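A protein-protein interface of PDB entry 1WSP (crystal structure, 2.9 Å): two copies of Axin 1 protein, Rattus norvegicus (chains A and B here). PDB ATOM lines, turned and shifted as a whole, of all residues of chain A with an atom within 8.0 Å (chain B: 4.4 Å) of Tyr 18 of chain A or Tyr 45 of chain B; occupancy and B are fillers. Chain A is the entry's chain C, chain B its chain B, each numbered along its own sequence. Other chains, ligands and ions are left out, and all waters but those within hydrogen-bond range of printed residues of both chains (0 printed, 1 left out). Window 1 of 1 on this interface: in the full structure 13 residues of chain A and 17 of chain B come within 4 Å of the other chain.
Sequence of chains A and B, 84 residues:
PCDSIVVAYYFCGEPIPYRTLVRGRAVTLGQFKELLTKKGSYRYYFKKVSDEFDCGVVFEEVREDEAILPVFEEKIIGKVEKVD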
ATOM      1  N   VAL A   6      14.672  -7.604  39.494  1.00  0.00           N
ATOM      2  CA  VAL A   6      14.204  -8.231  38.262  1.00  0.00           C
ATOM      3  C   VAL A   6      13.291  -7.282  37.497  1.00  0.00           C
ATOM      4  O   VAL A   6      12.317  -6.751  38.035  1.00  0.00           O
ATOM      5  CB  VAL A   6      13.446  -9.569  38.533  1.00  0.00           C
ATOM      6  CG1 VAL A   6      12.888 -10.130  37.226  1.00  0.00           C
ATOM      7  CG2 VAL A   6      14.399 -10.596  39.163  1.00  0.00           C
ATOM      8  N   VAL A   7      13.632  -7.070  36.233  1.00  0.00           N
ATOM      9  CA  VAL A   7      12.858  -6.219  35.365  1.00  0.00           C
ATOM     10  C   VAL A   7      12.439  -7.003  34.128  1.00  0.00           C
ATOM     11  O   VAL A   7      13.274  -7.358  33.292  1.00  0.00           O
ATOM     12  CB  VAL A   7      13.680  -4.983  34.972  1.00  0.00           C
ATOM     13  CG1 VAL A   7      12.983  -4.232  33.848  1.00  0.00           C
ATOM     14  CG2 VAL A   7      13.861  -4.092  36.201  1.00  0.00           C
ATOM     15  N   ALA A   8      11.143  -7.290  34.033  1.00  0.00           N
ATOM     16  CA  ALA A   8      10.574  -7.972  32.870  1.00  0.00           C
ATOM     17  C   ALA A   8       9.569  -7.057  32.192  1.00  0.00           C
ATOM     18  O   ALA A   8       8.761  -6.424  32.866  1.00  0.00           O
ATOM     19  CB  ALA A   8       9.886  -9.251  33.304  1.00  0.00           C
ATOM     20  N   TYR A   9       9.596  -6.976  30.870  1.00  0.00           N
ATOM     21  CA  TYR A   9       8.503  -6.287  30.199  1.00  0.00           C
ATOM     22  C   TYR A   9       7.975  -7.061  29.011  1.00  0.00           C
ATOM     23  O   TYR A   9       8.732  -7.722  28.293  1.00  0.00           O
ATOM     24  CB  TYR A   9       8.924  -4.887  29.754  1.00  0.00           C
ATOM     25  CG  TYR A   9      10.135  -4.879  28.871  1.00  0.00           C
ATOM     26  CD1 TYR A   9      10.005  -4.920  27.480  1.00  0.00           C
ATOM     27  CD2 TYR A   9      11.415  -4.867  29.417  1.00  0.00           C
ATOM     28  CE1 TYR A   9      11.119  -4.960  26.660  1.00  0.00           C
ATOM     29  CE2 TYR A   9      12.532  -4.904  28.604  1.00  0.00           C
ATOM     30  CZ  TYR A   9      12.377  -4.954  27.228  1.00  0.00           C
ATOM     31  OH  TYR A   9      13.481  -5.045  26.423  1.00  0.00           O
ATOM     32  N   TYR A  10       6.659  -6.996  28.834  1.00  0.00           N
ATOM     33  CA  TYR A  10       6.010  -7.468  27.624  1.00  0.00           C
ATOM     34  C   TYR A  10       6.123  -6.386  26.574  1.00  0.00           C
ATOM     35  O   TYR A  10       5.819  -5.224  26.834  1.00  0.00           O
ATOM     36  CB  TYR A  10       4.559  -7.764  27.929  1.00  0.00           C
ATOM     37  CG  TYR A  10       4.408  -8.953  28.837  1.00  0.00           C
ATOM     38  CD1 TYR A  10       4.658  -8.852  30.208  1.00  0.00           C
ATOM     39  CD2 TYR A  10       4.043 -10.189  28.325  1.00  0.00           C
ATOM     40  CE1 TYR A  10       4.546  -9.968  31.051  1.00  0.00           C
ATOM     41  CE2 TYR A  10       3.928 -11.303  29.146  1.00  0.00           C
ATOM     42  CZ  TYR A  10       4.181 -11.193  30.507  1.00  0.00           C
ATOM     43  OH  TYR A  10       4.089 -12.325  31.296  1.00  0.00           O
ATOM     44  N   PHE A  11       6.571  -6.759  25.385  1.00  0.00           N
ATOM     45  CA  PHE A  11       6.912  -5.765  24.372  1.00  0.00           C
ATOM     46  C   PHE A  11       5.917  -5.843  23.207  1.00  0.00           C
ATOM     47  O   PHE A  11       5.795  -6.889  22.549  1.00  0.00           O
ATOM     48  CB  PHE A  11       8.345  -6.010  23.881  1.00  0.00           C
ATOM     49  CG  PHE A  11       8.828  -5.020  22.847  1.00  0.00           C
ATOM     50  CD1 PHE A  11       9.081  -5.428  21.539  1.00  0.00           C
ATOM     51  CD2 PHE A  11       9.048  -3.677  23.186  1.00  0.00           C
ATOM     52  CE1 PHE A  11       9.550  -4.519  20.593  1.00  0.00           C
ATOM     53  CE2 PHE A  11       9.511  -2.778  22.247  1.00  0.00           C
ATOM     54  CZ  PHE A  11       9.763  -3.202  20.945  1.00  0.00           C
ATOM     55  N   CYS A  12       5.189  -4.741  22.996  1.00  0.00           N
ATOM     56  CA  CYS A  12       4.156  -4.615  21.959  1.00  0.00           C
ATOM     57  C   CYS A  12       3.130  -5.735  21.778  1.00  0.00           C
ATOM     58  O   CYS A  12       2.548  -5.856  20.704  1.00  0.00           O
ATOM     59  CB  CYS A  12       4.816  -4.356  20.613  1.00  0.00           C
ATOM     60  SG  CYS A  12       5.616  -2.771  20.534  1.00  0.00           S
ATOM     61  N   GLU A  14       3.766  -9.085  22.010  1.00  0.00           N
ATOM     62  CA  GLU A  14       4.538 -10.313  22.067  1.00  0.00           C
ATOM     63  C   GLU A  14       4.191 -10.992  23.391  1.00  0.00           C
ATOM     64  O   GLU A  14       4.259 -10.363  24.450  1.00  0.00           O
ATOM     65  CB  GLU A  14       6.042  -9.985  22.025  1.00  0.00           C
ATOM     66  CG  GLU A  14       6.492  -9.183  20.784  1.00  0.00           C
ATOM     67  CD  GLU A  14       8.021  -9.113  20.631  1.00  0.00           C
ATOM     68  OE1 GLU A  14       8.716  -9.929  21.268  1.00  0.00           O
ATOM     69  OE2 GLU A  14       8.530  -8.247  19.877  1.00  0.00           O
ATOM     70  N   PRO A  15       3.751 -12.260  23.348  1.00  0.00           N
ATOM     71  CA  PRO A  15       3.431 -12.899  24.634  1.00  0.00           C
ATOM     72  C   PRO A  15       4.661 -12.984  25.554  1.00  0.00           C
ATOM     73  O   PRO A  15       4.713 -12.300  26.581  1.00  0.00           O
ATOM     74  CB  PRO A  15       2.875 -14.283  24.250  1.00  0.00           C
ATOM     75  CG  PRO A  15       3.187 -14.464  22.817  1.00  0.00           C
ATOM     76  CD  PRO A  15       3.339 -13.081  22.199  1.00  0.00           C
ATOM     77  N   ILE A  16       5.654 -13.788  25.172  1.00  0.00           N
ATOM     78  CA  ILE A  16       6.850 -13.983  25.996  1.00  0.00           C
ATOM     79  C   ILE A  16       7.563 -12.664  26.363  1.00  0.00           C
ATOM     80  O   ILE A  16       8.156 -11.994  25.504  1.00  0.00           O
ATOM     81  CB  ILE A  16       7.867 -14.883  25.277  1.00  0.00           C
ATOM     82  CG1 ILE A  16       7.281 -16.274  25.042  1.00  0.00           C
ATOM     83  CG2 ILE A  16       9.138 -14.980  26.096  1.00  0.00           C
ATOM     84  CD1 ILE A  16       8.296 -17.272  24.462  1.00  0.00           C
ATOM     85  N   PRO A  17       7.535 -12.293  27.654  1.00  0.00           N
ATOM     86  CA  PRO A  17       8.167 -11.070  28.138  1.00  0.00           C
ATOM     87  C   PRO A  17       9.677 -11.211  28.130  1.00  0.00           C
ATOM     88  O   PRO A  17      10.191 -12.313  28.186  1.00  0.00           O
ATOM     89  CB  PRO A  17       7.614 -10.932  29.551  1.00  0.00           C
ATOM     90  CG  PRO A  17       7.396 -12.339  29.987  1.00  0.00           C
ATOM     91  CD  PRO A  17       6.960 -13.077  28.763  1.00  0.00           C
ATOM     92  N   TYR A  18      10.387 -10.093  28.068  1.00  0.00           N
ATOM     93  CA  TYR A  18      11.852 -10.116  28.098  1.00  0.00           C
ATOM     94  C   TYR A  18      12.344  -9.844  29.523  1.00  0.00           C
ATOM     95  O   TYR A  18      11.905  -8.886  30.160  1.00  0.00           O
ATOM     96  CB  TYR A  18      12.437  -9.056  27.139  1.00  0.00           C
ATOM     97  CG  TYR A  18      12.181  -9.286  25.660  1.00  0.00           C
ATOM     98  CD1 TYR A  18      10.900  -9.605  25.189  1.00  0.00           C
ATOM     99  CD2 TYR A  18      13.209  -9.147  24.727  1.00  0.00           C
ATOM    100  CE1 TYR A  18      10.648  -9.774  23.816  1.00  0.00           C
ATOM    101  CE2 TYR A  18      12.972  -9.313  23.359  1.00  0.00           C
ATOM    102  CZ  TYR A  18      11.690  -9.621  22.907  1.00  0.00           C
ATOM    103  OH  TYR A  18      11.452  -9.740  21.557  1.00  0.00           O
ATOM    104  N   ARG A  19      13.252 -10.681  30.019  1.00  0.00           N
ATOM    105  CA  ARG A  19      13.655 -10.623  31.420  1.00  0.00           C
ATOM    106  C   ARG A  19      15.107 -10.188  31.601  1.00  0.00           C
ATOM    107  O   ARG A  19      16.006 -10.661  30.904  1.00  0.00           O
ATOM    108  CB  ARG A  19      13.452 -11.987  32.072  1.00  0.00           C
ATOM    109  CG  ARG A  19      13.622 -11.971  33.573  1.00  0.00           C
ATOM    110  CD  ARG A  19      12.969 -13.193  34.144  1.00  0.00           C
ATOM    111  NE  ARG A  19      13.379 -13.482  35.511  1.00  0.00           N
ATOM    112  CZ  ARG A  19      14.624 -13.378  35.972  1.00  0.00           C
ATOM    113  NH1 ARG A  19      15.614 -12.976  35.175  1.00  0.00           N
ATOM    114  NH2 ARG A  19      14.883 -13.707  37.232  1.00  0.00           N
ATOM    115  N   THR A  20      15.340  -9.279  32.539  1.00  0.00           N
ATOM    116  CA  THR A  20      16.709  -8.904  32.883  1.00  0.00           C
ATOM    117  C   THR A  20      16.802  -8.524  34.354  1.00  0.00           C
ATOM    118  O   THR A  20      15.800  -8.201  34.987  1.00  0.00           O
ATOM    119  CB  THR A  20      17.212  -7.711  32.031  1.00  0.00           C
ATOM    120  OG1 THR A  20      18.640  -7.640  32.095  1.00  0.00           O
ATOM    121  CG2 THR A  20      16.642  -6.403  32.553  1.00  0.00           C
ATOM    122  N   LEU A  21      18.015  -8.574  34.891  1.00  0.00           N
ATOM    123  CA  LEU A  21      18.275  -8.088  36.234  1.00  0.00           C
ATOM    124  C   LEU A  21      18.997  -6.761  36.190  1.00  0.00           C
ATOM    125  O   LEU A  21      19.889  -6.550  35.363  1.00  0.00           O
ATOM    126  CB  LEU A  21      19.114  -9.098  37.012  1.00  0.00           C
ATOM    127  CG  LEU A  21      18.297 -10.171  37.736  1.00  0.00           C
ATOM    128  CD1 LEU A  21      17.179 -10.721  36.822  1.00  0.00           C
ATOM    129  CD2 LEU A  21      19.245 -11.271  38.193  1.00  0.00           C
ATOM    130  N   PHE A  32      15.048   2.024  32.804  1.00  0.00           N
ATOM    131  CA  PHE A  32      14.260   1.010  32.122  1.00  0.00           C
ATOM    132  C   PHE A  32      14.325   1.281  30.634  1.00  0.00           C
ATOM    133  O   PHE A  32      14.347   0.356  29.821  1.00  0.00           O
ATOM    134  CB  PHE A  32      12.810   1.067  32.593  1.00  0.00           C
ATOM    135  CG  PHE A  32      11.910   0.068  31.921  1.00  0.00           C
ATOM    136  CD1 PHE A  32      11.925  -1.270  32.303  1.00  0.00           C
ATOM    137  CD2 PHE A  32      11.031   0.468  30.916  1.00  0.00           C
ATOM    138  CE1 PHE A  32      11.082  -2.196  31.700  1.00  0.00           C
ATOM    139  CE2 PHE A  32      10.181  -0.453  30.304  1.00  0.00           C
ATOM    140  CZ  PHE A  32      10.208  -1.790  30.699  1.00  0.00           C
ATOM    141  N   GLU A  34      16.673   2.397  28.960  1.00  0.00           N
ATOM    142  CA  GLU A  34      17.967   2.057  28.377  1.00  0.00           C
ATOM    143  C   GLU A  34      18.090   0.575  28.009  1.00  0.00           C
ATOM    144  O   GLU A  34      19.003   0.183  27.276  1.00  0.00           O
ATOM    145  CB  GLU A  34      19.087   2.439  29.341  1.00  0.00           C
ATOM    146  CG  GLU A  34      19.096   3.907  29.717  1.00  0.00           C
ATOM    147  CD  GLU A  34      20.079   4.221  30.830  1.00  0.00           C
ATOM    148  OE1 GLU A  34      21.236   4.584  30.522  1.00  0.00           O
ATOM    149  OE2 GLU A  34      19.689   4.105  32.013  1.00  0.00           O
ATOM    150  N   LEU A  35      17.174  -0.243  28.519  1.00  0.00           N
ATOM    151  CA  LEU A  35      17.160  -1.658  28.180  1.00  0.00           C
ATOM    152  C   LEU A  35      16.482  -1.896  26.841  1.00  0.00           C
ATOM    153  O   LEU A  35      16.701  -2.920  26.205  1.00  0.00           O
ATOM    154  CB  LEU A  35      16.440  -2.460  29.266  1.00  0.00           C
ATOM    155  CG  LEU A  35      17.177  -2.796  30.567  1.00  0.00           C
ATOM    156  CD1 LEU A  35      18.091  -1.661  30.971  1.00  0.00           C
ATOM    157  CD2 LEU A  35      16.160  -3.073  31.643  1.00  0.00           C
ATOM    158  N   LEU A  36      15.657  -0.946  26.414  1.00  0.00           N
ATOM    159  CA  LEU A  36      14.898  -1.089  25.179  1.00  0.00           C
ATOM    160  C   LEU A  36      15.807  -0.876  23.955  1.00  0.00           C
ATOM    161  O   LEU A  36      16.690  -0.017  23.977  1.00  0.00           O
ATOM    162  CB  LEU A  36      13.740  -0.085  25.183  1.00  0.00           C
ATOM    163  CG  LEU A  36      12.811  -0.109  26.411  1.00  0.00           C
ATOM    164  CD1 LEU A  36      11.881   1.076  26.369  1.00  0.00           C
ATOM    165  CD2 LEU A  36      12.004  -1.391  26.458  1.00  0.00           C
ATOM    166  N   THR A  37      15.604  -1.666  22.899  1.00  0.00           N
ATOM    167  CA  THR A  37      16.532  -1.679  21.763  1.00  0.00           C
ATOM    168  C   THR A  37      16.003  -0.947  20.548  1.00  0.00           C
ATOM    169  O   THR A  37      16.776  -0.524  19.694  1.00  0.00           O
ATOM    170  CB  THR A  37      16.893  -3.120  21.309  1.00  0.00           C
ATOM    171  OG1 THR A  37      15.698  -3.836  20.968  1.00  0.00           O
ATOM    172  CG2 THR A  37      17.666  -3.851  22.400  1.00  0.00           C
ATOM    173  N   LYS A  38      14.685  -0.805  20.474  1.00  0.00           N
ATOM    174  CA  LYS A  38      14.039  -0.232  19.294  1.00  0.00           C
ATOM    175  C   LYS A  38      13.638   1.239  19.496  1.00  0.00           C
ATOM    176  O   LYS A  38      13.023   1.601  20.502  1.00  0.00           O
ATOM    177  CB  LYS A  38      12.799  -1.062  18.924  1.00  0.00           C
ATOM    178  CG  LYS A  38      13.055  -2.550  18.758  1.00  0.00           C
ATOM    179  CD  LYS A  38      13.894  -2.833  17.535  1.00  0.00           C
ATOM    180  CE  LYS A  38      14.660  -4.129  17.705  1.00  0.00           C
ATOM    181  NZ  LYS A  38      16.138  -3.919  17.614  1.00  0.00           N
ATOM    182  N   ILE A  76       9.610  -5.960  38.802  1.00  0.00           N
ATOM    183  CA  ILE A  76       9.082  -4.903  37.959  1.00  0.00           C
ATOM    184  C   ILE A  76       8.496  -5.503  36.679  1.00  0.00           C
ATOM    185  O   ILE A  76       9.213  -6.008  35.833  1.00  0.00           O
ATOM    186  CB  ILE A  76      10.201  -3.883  37.627  1.00  0.00           C
ATOM    187  CG1 ILE A  76      10.473  -3.014  38.861  1.00  0.00           C
ATOM    188  CG2 ILE A  76       9.834  -3.053  36.410  1.00  0.00           C
ATOM    189  CD1 ILE A  76      11.750  -2.181  38.775  1.00  0.00           C
ATOM    190  N   GLY A  78       6.603  -4.657  33.369  1.00  0.00           N
ATOM    191  CA  GLY A  78       6.227  -3.570  32.483  1.00  0.00           C
ATOM    192  C   GLY A  78       5.512  -4.009  31.218  1.00  0.00           C
ATOM    193  O   GLY A  78       5.745  -5.110  30.709  1.00  0.00           O
ATOM    194  N   ARG B  43      21.702  -6.530  21.912  1.00  0.00           N
ATOM    195  CA  ARG B  43      21.311  -7.257  23.113  1.00  0.00           C
ATOM    196  C   ARG B  43      20.930  -8.682  22.728  1.00  0.00           C
ATOM    197  O   ARG B  43      20.521  -8.943  21.594  1.00  0.00           O
ATOM    198  CB  ARG B  43      20.134  -6.562  23.802  1.00  0.00           C
ATOM    199  CG  ARG B  43      20.491  -5.204  24.360  1.00  0.00           C
ATOM    200  CD  ARG B  43      19.472  -4.760  25.368  1.00  0.00           C
ATOM    201  NE  ARG B  43      20.090  -4.395  26.634  1.00  0.00           N
ATOM    202  CZ  ARG B  43      20.271  -3.146  27.043  1.00  0.00           C
ATOM    203  NH1 ARG B  43      19.884  -2.134  26.271  1.00  0.00           N
ATOM    204  NH2 ARG B  43      20.805  -2.907  28.239  1.00  0.00           N
ATOM    205  N   TYR B  44      21.071  -9.605  23.671  1.00  0.00           N
ATOM    206  CA  TYR B  44      20.877 -11.011  23.370  1.00  0.00           C
ATOM    207  C   TYR B  44      19.915 -11.618  24.367  1.00  0.00           C
ATOM    208  O   TYR B  44      20.082 -11.460  25.566  1.00  0.00           O
ATOM    209  CB  TYR B  44      22.224 -11.740  23.425  1.00  0.00           C
ATOM    210  CG  TYR B  44      23.338 -10.979  22.743  1.00  0.00           C
ATOM    211  CD1 TYR B  44      24.137 -10.094  23.467  1.00  0.00           C
ATOM    212  CD2 TYR B  44      23.603 -11.145  21.376  1.00  0.00           C
ATOM    213  CE1 TYR B  44      25.181  -9.391  22.858  1.00  0.00           C
ATOM    214  CE2 TYR B  44      24.649 -10.447  20.751  1.00  0.00           C
ATOM    215  CZ  TYR B  44      25.440  -9.576  21.508  1.00  0.00           C
ATOM    216  OH  TYR B  44      26.525  -8.933  20.951  1.00  0.00           O
ATOM    217  N   TYR B  45      18.903 -12.310  23.864  1.00  0.00           N
ATOM    218  CA  TYR B  45      17.929 -12.969  24.720  1.00  0.00           C
ATOM    219  C   TYR B  45      17.829 -14.438  24.343  1.00  0.00           C
ATOM    220  O   TYR B  45      18.070 -14.811  23.192  1.00  0.00           O
ATOM    221  CB  TYR B  45      16.561 -12.310  24.580  1.00  0.00           C
ATOM    222  CG  TYR B  45      16.608 -10.800  24.582  1.00  0.00           C
ATOM    223  CD1 TYR B  45      16.461 -10.078  25.762  1.00  0.00           C
ATOM    224  CD2 TYR B  45      16.736 -10.088  23.389  1.00  0.00           C
ATOM    225  CE1 TYR B  45      16.426  -8.682  25.747  1.00  0.00           C
ATOM    226  CE2 TYR B  45      16.708  -8.707  23.366  1.00  0.00           C
ATOM    227  CZ  TYR B  45      16.547  -8.011  24.544  1.00  0.00           C
ATOM    228  OH  TYR B  45      16.459  -6.645  24.506  1.00  0.00           O
ATOM    229  N   PHE B  46      17.477 -15.266  25.323  1.00  0.00           N
ATOM    230  CA  PHE B  46      17.344 -16.704  25.113  1.00  0.00           C
ATOM    231  C   PHE B  46      16.113 -17.264  25.852  1.00  0.00           C
ATOM    232  O   PHE B  46      15.925 -17.012  27.046  1.00  0.00           O
ATOM    233  CB  PHE B  46      18.627 -17.409  25.589  1.00  0.00           C
ATOM    234  CG  PHE B  46      19.863 -17.002  24.831  1.00  0.00           C
ATOM    235  CD1 PHE B  46      20.277 -17.719  23.714  1.00  0.00           C
ATOM    236  CD2 PHE B  46      20.584 -15.874  25.203  1.00  0.00           C
ATOM    237  CE1 PHE B  46      21.387 -17.312  22.972  1.00  0.00           C
ATOM    238  CE2 PHE B  46      21.688 -15.463  24.472  1.00  0.00           C
ATOM    239  CZ  PHE B  46      22.089 -16.186  23.350  1.00  0.00           C
ATOM    240  N   PHE B  59      12.305 -14.594  27.510  1.00  0.00           N
ATOM    241  CA  PHE B  59      13.564 -14.333  26.825  1.00  0.00           C
ATOM    242  C   PHE B  59      14.482 -13.646  27.813  1.00  0.00           C
ATOM    243  O   PHE B  59      14.381 -12.447  28.036  1.00  0.00           O
ATOM    244  CB  PHE B  59      13.357 -13.418  25.619  1.00  0.00           C
ATOM    245  CG  PHE B  59      12.846 -14.120  24.409  1.00  0.00           C
ATOM    246  CD1 PHE B  59      11.612 -13.776  23.864  1.00  0.00           C
ATOM    247  CD2 PHE B  59      13.583 -15.147  23.824  1.00  0.00           C
ATOM    248  CE1 PHE B  59      11.113 -14.449  22.749  1.00  0.00           C
ATOM    249  CE2 PHE B  59      13.098 -15.829  22.710  1.00  0.00           C
ATOM    250  CZ  PHE B  59      11.860 -15.482  22.171  1.00  0.00           C
ATOM    251  N   GLU B  60      15.367 -14.433  28.409  1.00  0.00           N
ATOM    252  CA  GLU B  60      16.357 -13.938  29.356  1.00  0.00           C
ATOM    253  C   GLU B  60      17.427 -13.139  28.632  1.00  0.00           C
ATOM    254  O   GLU B  60      18.058 -13.633  27.694  1.00  0.00           O
ATOM    255  CB  GLU B  60      17.023 -15.114  30.069  1.00  0.00           C
ATOM    256  CG  GLU B  60      16.429 -15.454  31.405  1.00  0.00           C
ATOM    257  CD  GLU B  60      17.151 -14.759  32.521  1.00  0.00           C
ATOM    258  OE1 GLU B  60      18.390 -14.920  32.601  1.00  0.00           O
ATOM    259  OE2 GLU B  60      16.479 -14.049  33.302  1.00  0.00           O
ATOM    260  N   GLU B  61      17.638 -11.906  29.073  1.00  0.00           N
ATOM    261  CA  GLU B  61      18.709 -11.097  28.519  1.00  0.00           C
ATOM    262  C   GLU B  61      20.030 -11.551  29.135  1.00  0.00           C
ATOM    263  O   GLU B  61      20.153 -11.629  30.356  1.00  0.00           O
ATOM    264  CB  GLU B  61      18.470  -9.612  28.820  1.00  0.00           C
ATOM    265  CG  GLU B  61      19.314  -8.655  27.962  1.00  0.00           C
ATOM    266  CD  GLU B  61      19.757  -7.405  28.715  1.00  0.00           C
ATOM    267  OE1 GLU B  61      20.981  -7.226  28.888  1.00  0.00           O
ATOM    268  OE2 GLU B  61      18.886  -6.601  29.129  1.00  0.00           O
ATOM    269  N   ILE B  77      17.745 -21.314  22.014  1.00  0.00           N
ATOM    270  CA  ILE B  77      17.000 -20.420  21.150  1.00  0.00           C
ATOM    271  C   ILE B  77      17.255 -18.959  21.517  1.00  0.00           C
ATOM    272  O   ILE B  77      16.791 -18.464  22.555  1.00  0.00           O
ATOM    273  CB  ILE B  77      15.514 -20.653  21.274  1.00  0.00           C
ATOM    274  CG1 ILE B  77      15.185 -22.119  21.029  1.00  0.00           C
ATOM    275  CG2 ILE B  77      14.792 -19.792  20.256  1.00  0.00           C
ATOM    276  CD1 ILE B  77      13.735 -22.455  21.322  1.00  0.00           C
ATOM    277  N   GLY B  78      17.980 -18.263  20.649  1.00  0.00           N
ATOM    278  CA  GLY B  78      18.327 -16.884  20.929  1.00  0.00           C
ATOM    279  C   GLY B  78      17.611 -15.869  20.059  1.00  0.00           C
ATOM    280  O   GLY B  78      17.246 -16.157  18.915  1.00  0.00           O
ATOM    281  N   LYS B  79      17.416 -14.679  20.622  1.00  0.00           N
ATOM    282  CA  LYS B  79      16.918 -13.514  19.895  1.00  0.00           C
ATOM    283  C   LYS B  79      18.020 -12.468  19.894  1.00  0.00           C
ATOM    284  O   LYS B  79      18.473 -12.041  20.955  1.00  0.00           O
ATOM    285  CB  LYS B  79      15.681 -12.952  20.601  1.00  0.00           C
ATOM    286  CG  LYS B  79      14.594 -12.452  19.673  1.00  0.00           C
ATOM    287  CD  LYS B  79      13.225 -12.603  20.308  1.00  0.00           C
ATOM    288  CE  LYS B  79      12.133 -11.995  19.421  1.00  0.00           C
ATOM    289  NZ  LYS B  79      12.412 -10.574  19.004  1.00  0.00           N
ATOM    290  N   GLU B  81      18.994  -8.708  18.875  1.00  0.00           N
ATOM    291  CA  GLU B  81      18.450  -7.414  18.485  1.00  0.00           C
ATOM    292  C   GLU B  81      19.536  -6.347  18.412  1.00  0.00           C
ATOM    293  O   GLU B  81      20.277  -6.141  19.371  1.00  0.00           O
ATOM    294  CB  GLU B  81      17.384  -6.972  19.486  1.00  0.00           C
ATOM    295  CG  GLU B  81      16.190  -7.889  19.573  1.00  0.00           C
ATOM    296  CD  GLU B  81      15.442  -7.993  18.263  1.00  0.00           C
ATOM    297  OE1 GLU B  81      15.254  -6.959  17.583  1.00  0.00           O
ATOM    298  OE2 GLU B  81      15.037  -9.122  17.912  1.00  0.00           O
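OH of Tyr 18 of chain A is in hydrogen-bond range of NZ of Lys 79 of chain B (2.9 Å).
O of Arg 19 of chain A lies within hydrogen-bond range of N of Glu 61 of chain B.
The side-chain carboxylate of Glu 61 of chain B sits at hydrogen-bond distance from the side-chain hydroxyl of Thr 20 of chain A (3.2 Å).
The side-chain amino group of Lys 38 of chain A is in salt-bridge range of the side-chain carboxylate of Glu 81 of chain B, at 3.2 Å.
The backbone carbonyl oxygen (O) of Phe 59 of chain B sits at hydrogen-bond distance from the backbone NH (N) of Arg 19 of chain A.
The backbone NH (N) of Phe 59 of chain B lies within hydrogen-bond range of the backbone carbonyl oxygen (O) of Pro 17 of chain A (3.2 Å).
O of Glu 34 of chain A sits at hydrogen-bond distance from NH1 of Arg 43 of chain B.
NH1 of Arg 43 of chain B is in hydrogen-bond range of O of Leu 35 of chain A (3.3 Å).
OE2 of Glu 60 of chain B lies within salt-bridge range of NE of Arg 19 of chain A (3.8 Å).
The backbone carbonyl oxygen (O) of Glu 60 of chain B lies within hydrogen-bond range of the backbone NH (N) of Phe 46 of chain B (2.9 Å).
The backbone NH of Lys 79 of chain B sits at hydrogen-bond distance from the backbone carbonyl oxygen of Tyr 45 of chain B, at 2.7 Å.
NZ of Lys 38 of chain A lies within hydrogen-bond range of OG1 of Thr 37 of chain A, 3.4 Å away.
The backbone NH of Val 7 of chain A is in hydrogen-bond range of the backbone carbonyl oxygen of Thr 20 of chain A (2.7 Å).
O of Tyr 9 of chain A lies within hydrogen-bond range of N of Tyr 18 of chain A, 2.9 Å away.
The backbone NH (N) of Arg 43 of chain B lies within hydrogen-bond range of the backbone carbonyl oxygen (O) of Glu 81 of chain B.
Among the printed residues, merely in contact across the chains: Tyr 9 of chain A with Tyr 45 of chain B, Ile 16 of chain A with Phe 59 of chain B, Tyr 18 of chain A with Tyr 45 of chain B, Tyr 18 of chain A with Phe 59 of chain B, Thr 37 of chain A with Arg 43 of chain B, Thr 37 of chain A with Tyr 45 of chain B and Thr 37 of chain A with Glu 81 of chain B.
Tyr 18 of chain A touches three residues of chain B.
Of the printed residues of chain A, Arg 43 of chain B touches Glu 34, Leu 35 and Thr 37.
Of chain A, only Tyr 9, Tyr 18 and Thr 37 come within 4 Å of Tyr 45 of chain B.
Gly 78 of chain B touches none of the printed residues of chain A.
Printed residues of chain A within 4 Å of Lys 79 of chain B: Tyr 18.
The nearest printed residue of chain B that does not touch Tyr 18 of chain A is Glu 81 of chain B (5.1 Å).
Hydrophobic or aromatic side chains of chain B within 4 Å of the printed part of chain A: Tyr 45 and Phe 59.
Among the printed residues, 16 pairs touch across the chains.
Position printed for both chains: 78.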
